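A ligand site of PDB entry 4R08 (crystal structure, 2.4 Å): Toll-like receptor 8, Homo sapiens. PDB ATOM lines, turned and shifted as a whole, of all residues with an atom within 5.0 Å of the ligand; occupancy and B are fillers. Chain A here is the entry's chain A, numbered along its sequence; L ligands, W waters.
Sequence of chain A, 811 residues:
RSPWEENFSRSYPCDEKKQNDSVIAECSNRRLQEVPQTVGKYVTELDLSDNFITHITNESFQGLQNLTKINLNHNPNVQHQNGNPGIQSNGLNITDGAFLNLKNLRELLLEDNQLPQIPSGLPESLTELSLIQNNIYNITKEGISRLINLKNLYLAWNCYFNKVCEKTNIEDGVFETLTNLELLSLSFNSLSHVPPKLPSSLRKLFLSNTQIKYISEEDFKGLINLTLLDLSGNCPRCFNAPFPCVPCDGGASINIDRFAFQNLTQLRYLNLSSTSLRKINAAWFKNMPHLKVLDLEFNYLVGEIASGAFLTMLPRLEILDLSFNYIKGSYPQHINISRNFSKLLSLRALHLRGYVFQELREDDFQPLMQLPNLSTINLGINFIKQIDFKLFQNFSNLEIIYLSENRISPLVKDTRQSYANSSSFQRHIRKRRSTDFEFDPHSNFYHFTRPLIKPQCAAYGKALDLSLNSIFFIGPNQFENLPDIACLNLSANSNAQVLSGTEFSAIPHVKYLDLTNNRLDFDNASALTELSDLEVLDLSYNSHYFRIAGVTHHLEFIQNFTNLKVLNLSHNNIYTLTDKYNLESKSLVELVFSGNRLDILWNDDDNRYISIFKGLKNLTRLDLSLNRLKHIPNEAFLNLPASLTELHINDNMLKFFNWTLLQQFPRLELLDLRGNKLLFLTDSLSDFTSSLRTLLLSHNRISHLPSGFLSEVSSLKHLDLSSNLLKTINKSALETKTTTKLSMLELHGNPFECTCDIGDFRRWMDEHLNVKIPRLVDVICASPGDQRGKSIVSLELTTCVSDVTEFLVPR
A ring nitrogen (NE2) of His 447 sits at hydrogen-bond distance from an oxygen (O10) of the ligand. An oxygen (O14) of the ligand is in hydrogen-bond range of the backbone NH of Leu 452 (2.7 Å). O18 of the ligand is in hydrogen-bond range of NE of Arg 353. A nitrogen (N7) of the ligand lies within hydrogen-bond range of the side-chain carboxylate (OD1) of Asp 321 (2.7 Å). A nitrogen (N1) of the ligand sits at hydrogen-bond distance from the side-chain carboxylate (OE1) of Glu 318 (2.9 Å). A nitrogen (N6) of the ligand lies close to a ring nitrogen (NE2) of His 351.
The backbone NH (N) of His 447 sits at hydrogen-bond distance from the side-chain amide oxygen (OD1) of Asn 444, at 3.0 Å. A ring nitrogen (ND1) of His 447 lies within hydrogen-bond range of the side-chain carboxylate (OE2) of Glu 297, 3.1 Å away. The guanidinium group of Arg 353 sits close to the side-chain amide nitrogen of Asn 378 (3.4 Å). OG of Ser 323 sits at hydrogen-bond distance from OD2 of Asp 321 (2.6 Å). The side-chain carboxylate (OE2) of Glu 318 is in salt-bridge range of the guanidinium group (NH2) of Arg 348, 3.6 Å away. N of Ile 319 is in hydrogen-bond range of O of Lys 292, 3.0 Å away. O of Arg 348 sits at hydrogen-bond distance from N of Thr 376 (3.1 Å). NZ of Lys 292 is in hydrogen-bond range of OH of Tyr 269, at 3.5 Å.
Water W1 lies within hydrogen-bond range of O18 of the ligand (2.6 Å), OE2 of Glu 297 (2.9 Å) and OG of Ser 323 (3.1 Å). Water W2 bridges an oxygen (O11) of the ligand (2.8 Å) and a ring nitrogen (NE2) of His 351 (3.0 Å).
O17 of the ligand sits close to O of Arg 450 (3.5 Å). Merely in contact with the ligand: Lys 292 (3.9 Å), Val 293 (3.1 Å), Ile 319 (3.1 Å), Arg 348 (3.7 Å), Asn 378 (3.9 Å), Phe 448 (3.6 Å), Thr 449 (3.4 Å) and Pro 451 (3.3 Å). Hydrophobic or aromatic side chains that line the ligand: Val 293, Ile 319, His 351, His 447, Pro 451 and Leu 452. Within 4 Å of the ligand: Lys 292, Val 293, Glu 318, Ile 319, Asp 321, Arg 348, His 351, Arg 353, Asn 378, His 447, Phe 448, Thr 449, Arg 450, Pro 451 and Leu 452. Along chain A the residues within 4 Å of the ligand span positions 292 to 452.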
ATOM      1  N   TYR A 269       4.705  -3.097   0.641  1.00  0.00           N
ATOM      2  CA  TYR A 269       4.681  -4.119   1.686  1.00  0.00           C
ATOM      3  C   TYR A 269       3.748  -3.710   2.801  1.00  0.00           C
ATOM      4  O   TYR A 269       3.912  -2.660   3.347  1.00  0.00           O
ATOM      5  CB  TYR A 269       6.082  -4.285   2.308  1.00  0.00           C
ATOM      6  CG  TYR A 269       7.166  -4.550   1.294  1.00  0.00           C
ATOM      7  CD1 TYR A 269       7.788  -3.509   0.669  1.00  0.00           C
ATOM      8  CD2 TYR A 269       7.586  -5.849   1.010  1.00  0.00           C
ATOM      9  CE1 TYR A 269       8.787  -3.720  -0.243  1.00  0.00           C
ATOM     10  CE2 TYR A 269       8.610  -6.075   0.081  1.00  0.00           C
ATOM     11  CZ  TYR A 269       9.176  -4.988  -0.542  1.00  0.00           C
ATOM     12  OH  TYR A 269      10.181  -5.141  -1.459  1.00  0.00           O
ATOM     13  N   LYS A 292       2.948  -5.482  -3.405  1.00  0.00           N
ATOM     14  CA  LYS A 292       3.747  -6.660  -3.722  1.00  0.00           C
ATOM     15  C   LYS A 292       3.658  -7.769  -2.630  1.00  0.00           C
ATOM     16  O   LYS A 292       3.760  -8.926  -2.921  1.00  0.00           O
ATOM     17  CB  LYS A 292       5.203  -6.211  -3.804  1.00  0.00           C
ATOM     18  CG  LYS A 292       5.839  -6.350  -5.161  1.00  0.00           C
ATOM     19  CD  LYS A 292       7.358  -6.408  -5.016  1.00  0.00           C
ATOM     20  CE  LYS A 292       7.990  -5.105  -5.451  1.00  0.00           C
ATOM     21  NZ  LYS A 292       9.337  -4.949  -4.819  1.00  0.00           N
ATOM     22  N   VAL A 293       3.520  -7.379  -1.376  1.00  0.00           N
ATOM     23  CA  VAL A 293       3.571  -8.338  -0.285  1.00  0.00           C
ATOM     24  C   VAL A 293       2.476  -7.991   0.700  1.00  0.00           C
ATOM     25  O   VAL A 293       2.418  -6.894   1.221  1.00  0.00           O
ATOM     26  CB  VAL A 293       4.947  -8.298   0.420  1.00  0.00           C
ATOM     27  CG1 VAL A 293       4.991  -9.249   1.609  1.00  0.00           C
ATOM     28  CG2 VAL A 293       6.069  -8.652  -0.554  1.00  0.00           C
ATOM     29  N   GLU A 297      -0.646 -13.139   8.576  1.00  0.00           N
ATOM     30  CA  GLU A 297      -0.454 -14.263   9.469  1.00  0.00           C
ATOM     31  C   GLU A 297      -1.192 -14.036  10.751  1.00  0.00           C
ATOM     32  O   GLU A 297      -1.378 -12.923  11.161  1.00  0.00           O
ATOM     33  CB  GLU A 297       1.004 -14.395   9.793  1.00  0.00           C
ATOM     34  CG  GLU A 297       1.838 -14.720   8.566  1.00  0.00           C
ATOM     35  CD  GLU A 297       3.312 -14.499   8.805  1.00  0.00           C
ATOM     36  OE1 GLU A 297       3.795 -13.364   8.567  1.00  0.00           O
ATOM     37  OE2 GLU A 297       3.968 -15.477   9.268  1.00  0.00           O
ATOM     38  N   GLU A 318       2.705 -10.312  -5.267  1.00  0.00           N
ATOM     39  CA  GLU A 318       3.625 -11.432  -5.466  1.00  0.00           C
ATOM     40  C   GLU A 318       3.646 -12.419  -4.294  1.00  0.00           C
ATOM     41  O   GLU A 318       3.911 -13.600  -4.484  1.00  0.00           O
ATOM     42  CB  GLU A 318       5.035 -10.939  -5.676  1.00  0.00           C
ATOM     43  CG  GLU A 318       5.221 -10.215  -6.995  1.00  0.00           C
ATOM     44  CD  GLU A 318       6.540  -9.451  -7.089  1.00  0.00           C
ATOM     45  OE1 GLU A 318       7.279  -9.395  -6.082  1.00  0.00           O
ATOM     46  OE2 GLU A 318       6.811  -8.870  -8.170  1.00  0.00           O
ATOM     47  N   ILE A 319       3.426 -11.930  -3.075  1.00  0.00           N
ATOM     48  CA  ILE A 319       3.524 -12.759  -1.910  1.00  0.00           C
ATOM     49  C   ILE A 319       2.378 -12.555  -0.971  1.00  0.00           C
ATOM     50  O   ILE A 319       2.071 -11.435  -0.561  1.00  0.00           O
ATOM     51  CB  ILE A 319       4.851 -12.472  -1.202  1.00  0.00           C
ATOM     52  CG1 ILE A 319       5.960 -12.935  -2.159  1.00  0.00           C
ATOM     53  CG2 ILE A 319       4.935 -13.181   0.148  1.00  0.00           C
ATOM     54  CD1 ILE A 319       7.324 -12.781  -1.568  1.00  0.00           C
ATOM     55  N   ASP A 321       0.836 -14.179   2.539  1.00  0.00           N
ATOM     56  CA  ASP A 321       1.030 -15.058   3.658  1.00  0.00           C
ATOM     57  C   ASP A 321      -0.227 -15.089   4.476  1.00  0.00           C
ATOM     58  O   ASP A 321      -0.600 -14.094   5.074  1.00  0.00           O
ATOM     59  CB  ASP A 321       2.223 -14.596   4.499  1.00  0.00           C
ATOM     60  CG  ASP A 321       2.665 -15.669   5.490  1.00  0.00           C
ATOM     61  OD1 ASP A 321       3.869 -15.713   5.864  1.00  0.00           O
ATOM     62  OD2 ASP A 321       1.810 -16.514   5.835  1.00  0.00           O
ATOM     63  N   SER A 323      -0.705 -17.638   6.773  1.00  0.00           N
ATOM     64  CA  SER A 323      -0.352 -18.679   7.706  1.00  0.00           C
ATOM     65  C   SER A 323      -0.972 -18.475   9.090  1.00  0.00           C
ATOM     66  O   SER A 323      -1.297 -17.379   9.503  1.00  0.00           O
ATOM     67  CB  SER A 323       1.154 -18.777   7.776  1.00  0.00           C
ATOM     68  OG  SER A 323       1.688 -19.068   6.488  1.00  0.00           O
ATOM     69  N   ARG A 348       3.602 -15.006  -6.864  1.00  0.00           N
ATOM     70  CA  ARG A 348       4.781 -15.895  -6.925  1.00  0.00           C
ATOM     71  C   ARG A 348       4.780 -16.939  -5.791  1.00  0.00           C
ATOM     72  O   ARG A 348       5.004 -18.122  -6.042  1.00  0.00           O
ATOM     73  CB  ARG A 348       6.078 -15.083  -6.910  1.00  0.00           C
ATOM     74  CG  ARG A 348       6.135 -14.009  -7.975  1.00  0.00           C
ATOM     75  CD  ARG A 348       7.504 -13.831  -8.626  1.00  0.00           C
ATOM     76  NE  ARG A 348       7.477 -12.704  -9.563  1.00  0.00           N
ATOM     77  CZ  ARG A 348       8.511 -11.887  -9.848  1.00  0.00           C
ATOM     78  NH1 ARG A 348       9.700 -12.077  -9.292  1.00  0.00           N
ATOM     79  NH2 ARG A 348       8.339 -10.875 -10.697  1.00  0.00           N
ATOM     80  N   HIS A 351       1.783 -18.699   1.037  1.00  0.00           N
ATOM     81  CA  HIS A 351       2.028 -19.352   2.304  1.00  0.00           C
ATOM     82  C   HIS A 351       0.741 -19.581   3.049  1.00  0.00           C
ATOM     83  O   HIS A 351       0.063 -18.631   3.386  1.00  0.00           O
ATOM     84  CB  HIS A 351       2.962 -18.509   3.146  1.00  0.00           C
ATOM     85  CG  HIS A 351       4.260 -18.189   2.462  1.00  0.00           C
ATOM     86  ND1 HIS A 351       5.294 -19.087   2.367  1.00  0.00           N
ATOM     87  CD2 HIS A 351       4.704 -17.029   1.907  1.00  0.00           C
ATOM     88  CE1 HIS A 351       6.316 -18.508   1.754  1.00  0.00           C
ATOM     89  NE2 HIS A 351       5.973 -17.267   1.450  1.00  0.00           N
ATOM     90  N   ARG A 353       0.630 -22.029   5.937  1.00  0.00           N
ATOM     91  CA  ARG A 353       0.883 -22.881   7.065  1.00  0.00           C
ATOM     92  C   ARG A 353      -0.307 -22.734   7.966  1.00  0.00           C
ATOM     93  O   ARG A 353      -0.930 -21.670   7.980  1.00  0.00           O
ATOM     94  CB  ARG A 353       2.096 -22.436   7.847  1.00  0.00           C
ATOM     95  CG  ARG A 353       3.410 -22.481   7.111  1.00  0.00           C
ATOM     96  CD  ARG A 353       4.408 -21.713   7.940  1.00  0.00           C
ATOM     97  NE  ARG A 353       5.724 -21.676   7.330  1.00  0.00           N
ATOM     98  CZ  ARG A 353       6.621 -22.653   7.407  1.00  0.00           C
ATOM     99  NH1 ARG A 353       6.316 -23.806   8.004  1.00  0.00           N
ATOM    100  NH2 ARG A 353       7.789 -22.507   6.817  1.00  0.00           N
ATOM    101  N   THR A 376       5.910 -21.066  -5.765  1.00  0.00           N
ATOM    102  CA  THR A 376       6.045 -21.689  -4.457  1.00  0.00           C
ATOM    103  C   THR A 376       4.702 -21.824  -3.760  1.00  0.00           C
ATOM    104  O   THR A 376       3.977 -20.829  -3.600  1.00  0.00           O
ATOM    105  CB  THR A 376       6.888 -20.812  -3.562  1.00  0.00           C
ATOM    106  OG1 THR A 376       8.230 -20.744  -4.058  1.00  0.00           O
ATOM    107  CG2 THR A 376       6.847 -21.336  -2.144  1.00  0.00           C
ATOM    108  N   ASN A 378       3.261 -23.325   0.009  1.00  0.00           N
ATOM    109  CA  ASN A 378       3.776 -23.723   1.321  1.00  0.00           C
ATOM    110  C   ASN A 378       2.594 -24.102   2.200  1.00  0.00           C
ATOM    111  O   ASN A 378       1.789 -23.261   2.589  1.00  0.00           O
ATOM    112  CB  ASN A 378       4.569 -22.556   1.930  1.00  0.00           C
ATOM    113  CG  ASN A 378       4.896 -22.716   3.412  1.00  0.00           C
ATOM    114  OD1 ASN A 378       4.695 -23.767   4.039  1.00  0.00           O
ATOM    115  ND2 ASN A 378       5.407 -21.645   3.971  1.00  0.00           N
ATOM    116  N   ASN A 444      12.083 -10.978  11.173  1.00  0.00           N
ATOM    117  CA  ASN A 444      10.654 -11.117  11.144  1.00  0.00           C
ATOM    118  C   ASN A 444      10.200 -11.897  12.378  1.00  0.00           C
ATOM    119  O   ASN A 444      10.718 -12.969  12.660  1.00  0.00           O
ATOM    120  CB  ASN A 444      10.240 -11.859   9.869  1.00  0.00           C
ATOM    121  CG  ASN A 444       8.755 -11.759   9.590  1.00  0.00           C
ATOM    122  OD1 ASN A 444       7.936 -12.273  10.344  1.00  0.00           O
ATOM    123  ND2 ASN A 444       8.412 -11.188   8.453  1.00  0.00           N
ATOM    124  N   HIS A 447       7.334 -15.169  11.080  1.00  0.00           N
ATOM    125  CA  HIS A 447       7.938 -16.374  10.521  1.00  0.00           C
ATOM    126  C   HIS A 447       9.460 -16.338  10.478  1.00  0.00           C
ATOM    127  O   HIS A 447      10.096 -15.286  10.727  1.00  0.00           O
ATOM    128  CB  HIS A 447       7.399 -16.653   9.113  1.00  0.00           C
ATOM    129  CG  HIS A 447       7.556 -15.511   8.171  1.00  0.00           C
ATOM    130  ND1 HIS A 447       6.595 -14.535   8.034  1.00  0.00           N
ATOM    131  CD2 HIS A 447       8.555 -15.167   7.336  1.00  0.00           C
ATOM    132  CE1 HIS A 447       6.989 -13.650   7.138  1.00  0.00           C
ATOM    133  NE2 HIS A 447       8.178 -14.012   6.690  1.00  0.00           N
ATOM    134  N   PHE A 448      10.046 -17.503  10.199  1.00  0.00           N
ATOM    135  CA  PHE A 448      11.465 -17.625   9.854  1.00  0.00           C
ATOM    136  C   PHE A 448      11.668 -17.295   8.383  1.00  0.00           C
ATOM    137  O   PHE A 448      10.773 -17.472   7.592  1.00  0.00           O
ATOM    138  CB  PHE A 448      11.999 -19.032  10.159  1.00  0.00           C
ATOM    139  CG  PHE A 448      12.024 -19.358  11.620  1.00  0.00           C
ATOM    140  CD1 PHE A 448      12.826 -18.617  12.502  1.00  0.00           C
ATOM    141  CD2 PHE A 448      11.200 -20.341  12.151  1.00  0.00           C
ATOM    142  CE1 PHE A 448      12.820 -18.863  13.874  1.00  0.00           C
ATOM    143  CE2 PHE A 448      11.194 -20.604  13.513  1.00  0.00           C
ATOM    144  CZ  PHE A 448      11.995 -19.854  14.375  1.00  0.00           C
ATOM    145  N   THR A 449      12.818 -16.735   8.064  1.00  0.00           N
ATOM    146  CA  THR A 449      13.113 -16.308   6.726  1.00  0.00           C
ATOM    147  C   THR A 449      14.222 -17.107   6.066  1.00  0.00           C
ATOM    148  O   THR A 449      14.701 -16.717   5.008  1.00  0.00           O
ATOM    149  CB  THR A 449      13.511 -14.833   6.688  1.00  0.00           C
ATOM    150  OG1 THR A 449      14.476 -14.597   7.692  1.00  0.00           O
ATOM    151  CG2 THR A 449      12.287 -13.944   6.934  1.00  0.00           C
ATOM    152  N   ARG A 450      14.578 -18.264   6.626  1.00  0.00           N
ATOM    153  CA  ARG A 450      15.407 -19.180   5.845  1.00  0.00           C
ATOM    154  C   ARG A 450      14.673 -19.643   4.601  1.00  0.00           C
ATOM    155  O   ARG A 450      13.446 -19.618   4.537  1.00  0.00           O
ATOM    156  CB  ARG A 450      15.938 -20.379   6.653  1.00  0.00           C
ATOM    157  CG  ARG A 450      15.002 -20.989   7.680  1.00  0.00           C
ATOM    158  CD  ARG A 450      15.433 -22.406   8.036  1.00  0.00           C
ATOM    159  NE  ARG A 450      15.076 -23.349   6.955  1.00  0.00           N
ATOM    160  CZ  ARG A 450      14.354 -24.472   7.106  1.00  0.00           C
ATOM    161  NH1 ARG A 450      13.944 -24.871   8.309  1.00  0.00           N
ATOM    162  NH2 ARG A 450      14.067 -25.203   6.040  1.00  0.00           N
ATOM    163  N   PRO A 451      15.412 -20.008   3.575  1.00  0.00           N
ATOM    164  CA  PRO A 451      14.757 -20.594   2.414  1.00  0.00           C
ATOM    165  C   PRO A 451      14.012 -21.862   2.767  1.00  0.00           C
ATOM    166  O   PRO A 451      14.467 -22.626   3.628  1.00  0.00           O
ATOM    167  CB  PRO A 451      15.912 -20.926   1.481  1.00  0.00           C
ATOM    168  CG  PRO A 451      16.943 -19.900   1.834  1.00  0.00           C
ATOM    169  CD  PRO A 451      16.823 -19.707   3.325  1.00  0.00           C
ATOM    170  N   LEU A 452      12.898 -22.105   2.085  1.00  0.00           N
ATOM    171  CA  LEU A 452      12.109 -23.294   2.328  1.00  0.00           C
ATOM    172  C   LEU A 452      12.909 -24.560   2.007  1.00  0.00           C
ATOM    173  O   LEU A 452      12.861 -25.528   2.745  1.00  0.00           O
ATOM    174  CB  LEU A 452      10.791 -23.267   1.527  1.00  0.00           C
ATOM    175  CG  LEU A 452       9.730 -22.300   2.071  1.00  0.00           C
ATOM    176  CD1 LEU A 452       8.585 -22.202   1.089  1.00  0.00           C
ATOM    177  CD2 LEU A 452       9.236 -22.703   3.448  1.00  0.00           C
ATOM    178  N   ILE A 453      13.630 -24.526   0.900  1.00  0.00           N
ATOM    179  CA  ILE A 453      14.389 -25.679   0.401  1.00  0.00           C
ATOM    180  C   ILE A 453      15.825 -25.213   0.378  1.00  0.00           C
ATOM    181  O   ILE A 453      16.071 -24.089  -0.019  1.00  0.00           O
ATOM    182  CB  ILE A 453      13.982 -26.007  -1.058  1.00  0.00           C
ATOM    183  CG1 ILE A 453      12.483 -26.158  -1.167  1.00  0.00           C
ATOM    184  CG2 ILE A 453      14.647 -27.284  -1.568  1.00  0.00           C
ATOM    185  CD1 ILE A 453      11.940 -27.333  -0.414  1.00  0.00           C
HETATM  186  O1  LIG L   1       9.030 -12.645  -5.429  1.00  0.00           O
HETATM  187  C1  LIG L   1       9.244 -12.088  -4.324  1.00  0.00           C
HETATM  188  C2  LIG L   1      10.060 -12.726  -3.368  1.00  0.00           C
HETATM  189  C3  LIG L   1      10.297 -12.123  -2.131  1.00  0.00           C
HETATM  190  N1  LIG L   1       8.715 -10.863  -4.036  1.00  0.00           N
HETATM  191  C4  LIG L   1       8.964 -10.277  -2.812  1.00  0.00           C
HETATM  192  O2  LIG L   1       8.466  -9.180  -2.517  1.00  0.00           O
HETATM  193  N2  LIG L   1       9.763 -10.903  -1.835  1.00  0.00           N
HETATM  194  C5  LIG L   1       9.964 -10.253  -0.509  1.00  0.00           C
HETATM  195  C6  LIG L   1       9.381 -11.073   0.660  1.00  0.00           C
HETATM  196  O3  LIG L   1       8.743 -10.219   1.614  1.00  0.00           O
HETATM  197  O4  LIG L   1      11.356 -10.087  -0.217  1.00  0.00           O
HETATM  198  C7  LIG L   1      11.689 -10.692   1.058  1.00  0.00           C
HETATM  199  C8  LIG L   1      13.115 -11.218   1.031  1.00  0.00           C
HETATM  200  O5  LIG L   1      13.133 -12.629   0.809  1.00  0.00           O
HETATM  201  P1  LIG L   1      13.981 -13.365  -0.358  1.00  0.00           P
HETATM  202  O6  LIG L   1      14.846 -12.283  -0.980  1.00  0.00           O
HETATM  203  O7  LIG L   1      14.729 -14.468   0.392  1.00  0.00           O
HETATM  204  O8  LIG L   1      12.868 -13.915  -1.233  1.00  0.00           O
HETATM  205  C9  LIG L   1      10.601 -11.725   1.311  1.00  0.00           C
HETATM  206  O9  LIG L   1      10.419 -12.025   2.697  1.00  0.00           O
HETATM  207  P2  LIG L   1       9.640 -13.365   3.220  1.00  0.00           P
HETATM  208  O10 LIG L   1       9.623 -13.271   4.720  1.00  0.00           O
HETATM  209  O11 LIG L   1       8.314 -13.615   2.506  1.00  0.00           O
HETATM  210  O12 LIG L   1      10.503 -14.646   2.766  1.00  0.00           O
HETATM  211  C10 LIG L   1      11.882 -14.930   2.975  1.00  0.00           C
HETATM  212  C11 LIG L   1      12.023 -16.445   2.794  1.00  0.00           C
HETATM  213  C12 LIG L   1      11.447 -16.924   1.431  1.00  0.00           C
HETATM  214  P3  LIG L   1      11.299 -18.636   0.571  1.00  0.00           P
HETATM  215  O13 LIG L   1      10.863 -18.569  -1.026  1.00  0.00           O
HETATM  216  O14 LIG L   1      12.151 -20.040   0.545  1.00  0.00           O
HETATM  217  O15 LIG L   1       9.767 -18.952   1.314  1.00  0.00           O
HETATM  218  O16 LIG L   1      12.601 -17.536   0.884  1.00  0.00           O
HETATM  219  C13 LIG L   1      10.330 -17.866   2.020  1.00  0.00           C
HETATM  220  O17 LIG L   1      11.280 -16.958   3.898  1.00  0.00           O
HETATM  221  C14 LIG L   1      10.775 -18.210   3.454  1.00  0.00           C
HETATM  222  N3  LIG L   1       9.734 -18.680   4.391  1.00  0.00           N
HETATM  223  C15 LIG L   1       9.728 -19.828   5.104  1.00  0.00           C
HETATM  224  N4  LIG L   1       8.566 -19.925   5.843  1.00  0.00           N
HETATM  225  C16 LIG L   1       8.593 -18.035   4.690  1.00  0.00           C
HETATM  226  C17 LIG L   1       7.843 -18.823   5.563  1.00  0.00           C
HETATM  227  N5  LIG L   1       8.087 -16.873   4.248  1.00  0.00           N
HETATM  228  C18 LIG L   1       6.881 -16.469   4.657  1.00  0.00           C
HETATM  229  N6  LIG L   1       6.433 -15.288   4.169  1.00  0.00           N
HETATM  230  N7  LIG L   1       6.148 -17.174   5.541  1.00  0.00           N
HETATM  231  C19 LIG L   1       6.599 -18.360   5.992  1.00  0.00           C
HETATM  232  O18 LIG L   1       5.905 -19.039   6.798  1.00  0.00           O
HETATM  233  O   HOH W   1       3.943 -18.239   8.374  1.00  0.00           O
HETATM  234  O   HOH W   2       8.192 -15.481   0.379  1.00  0.00           O
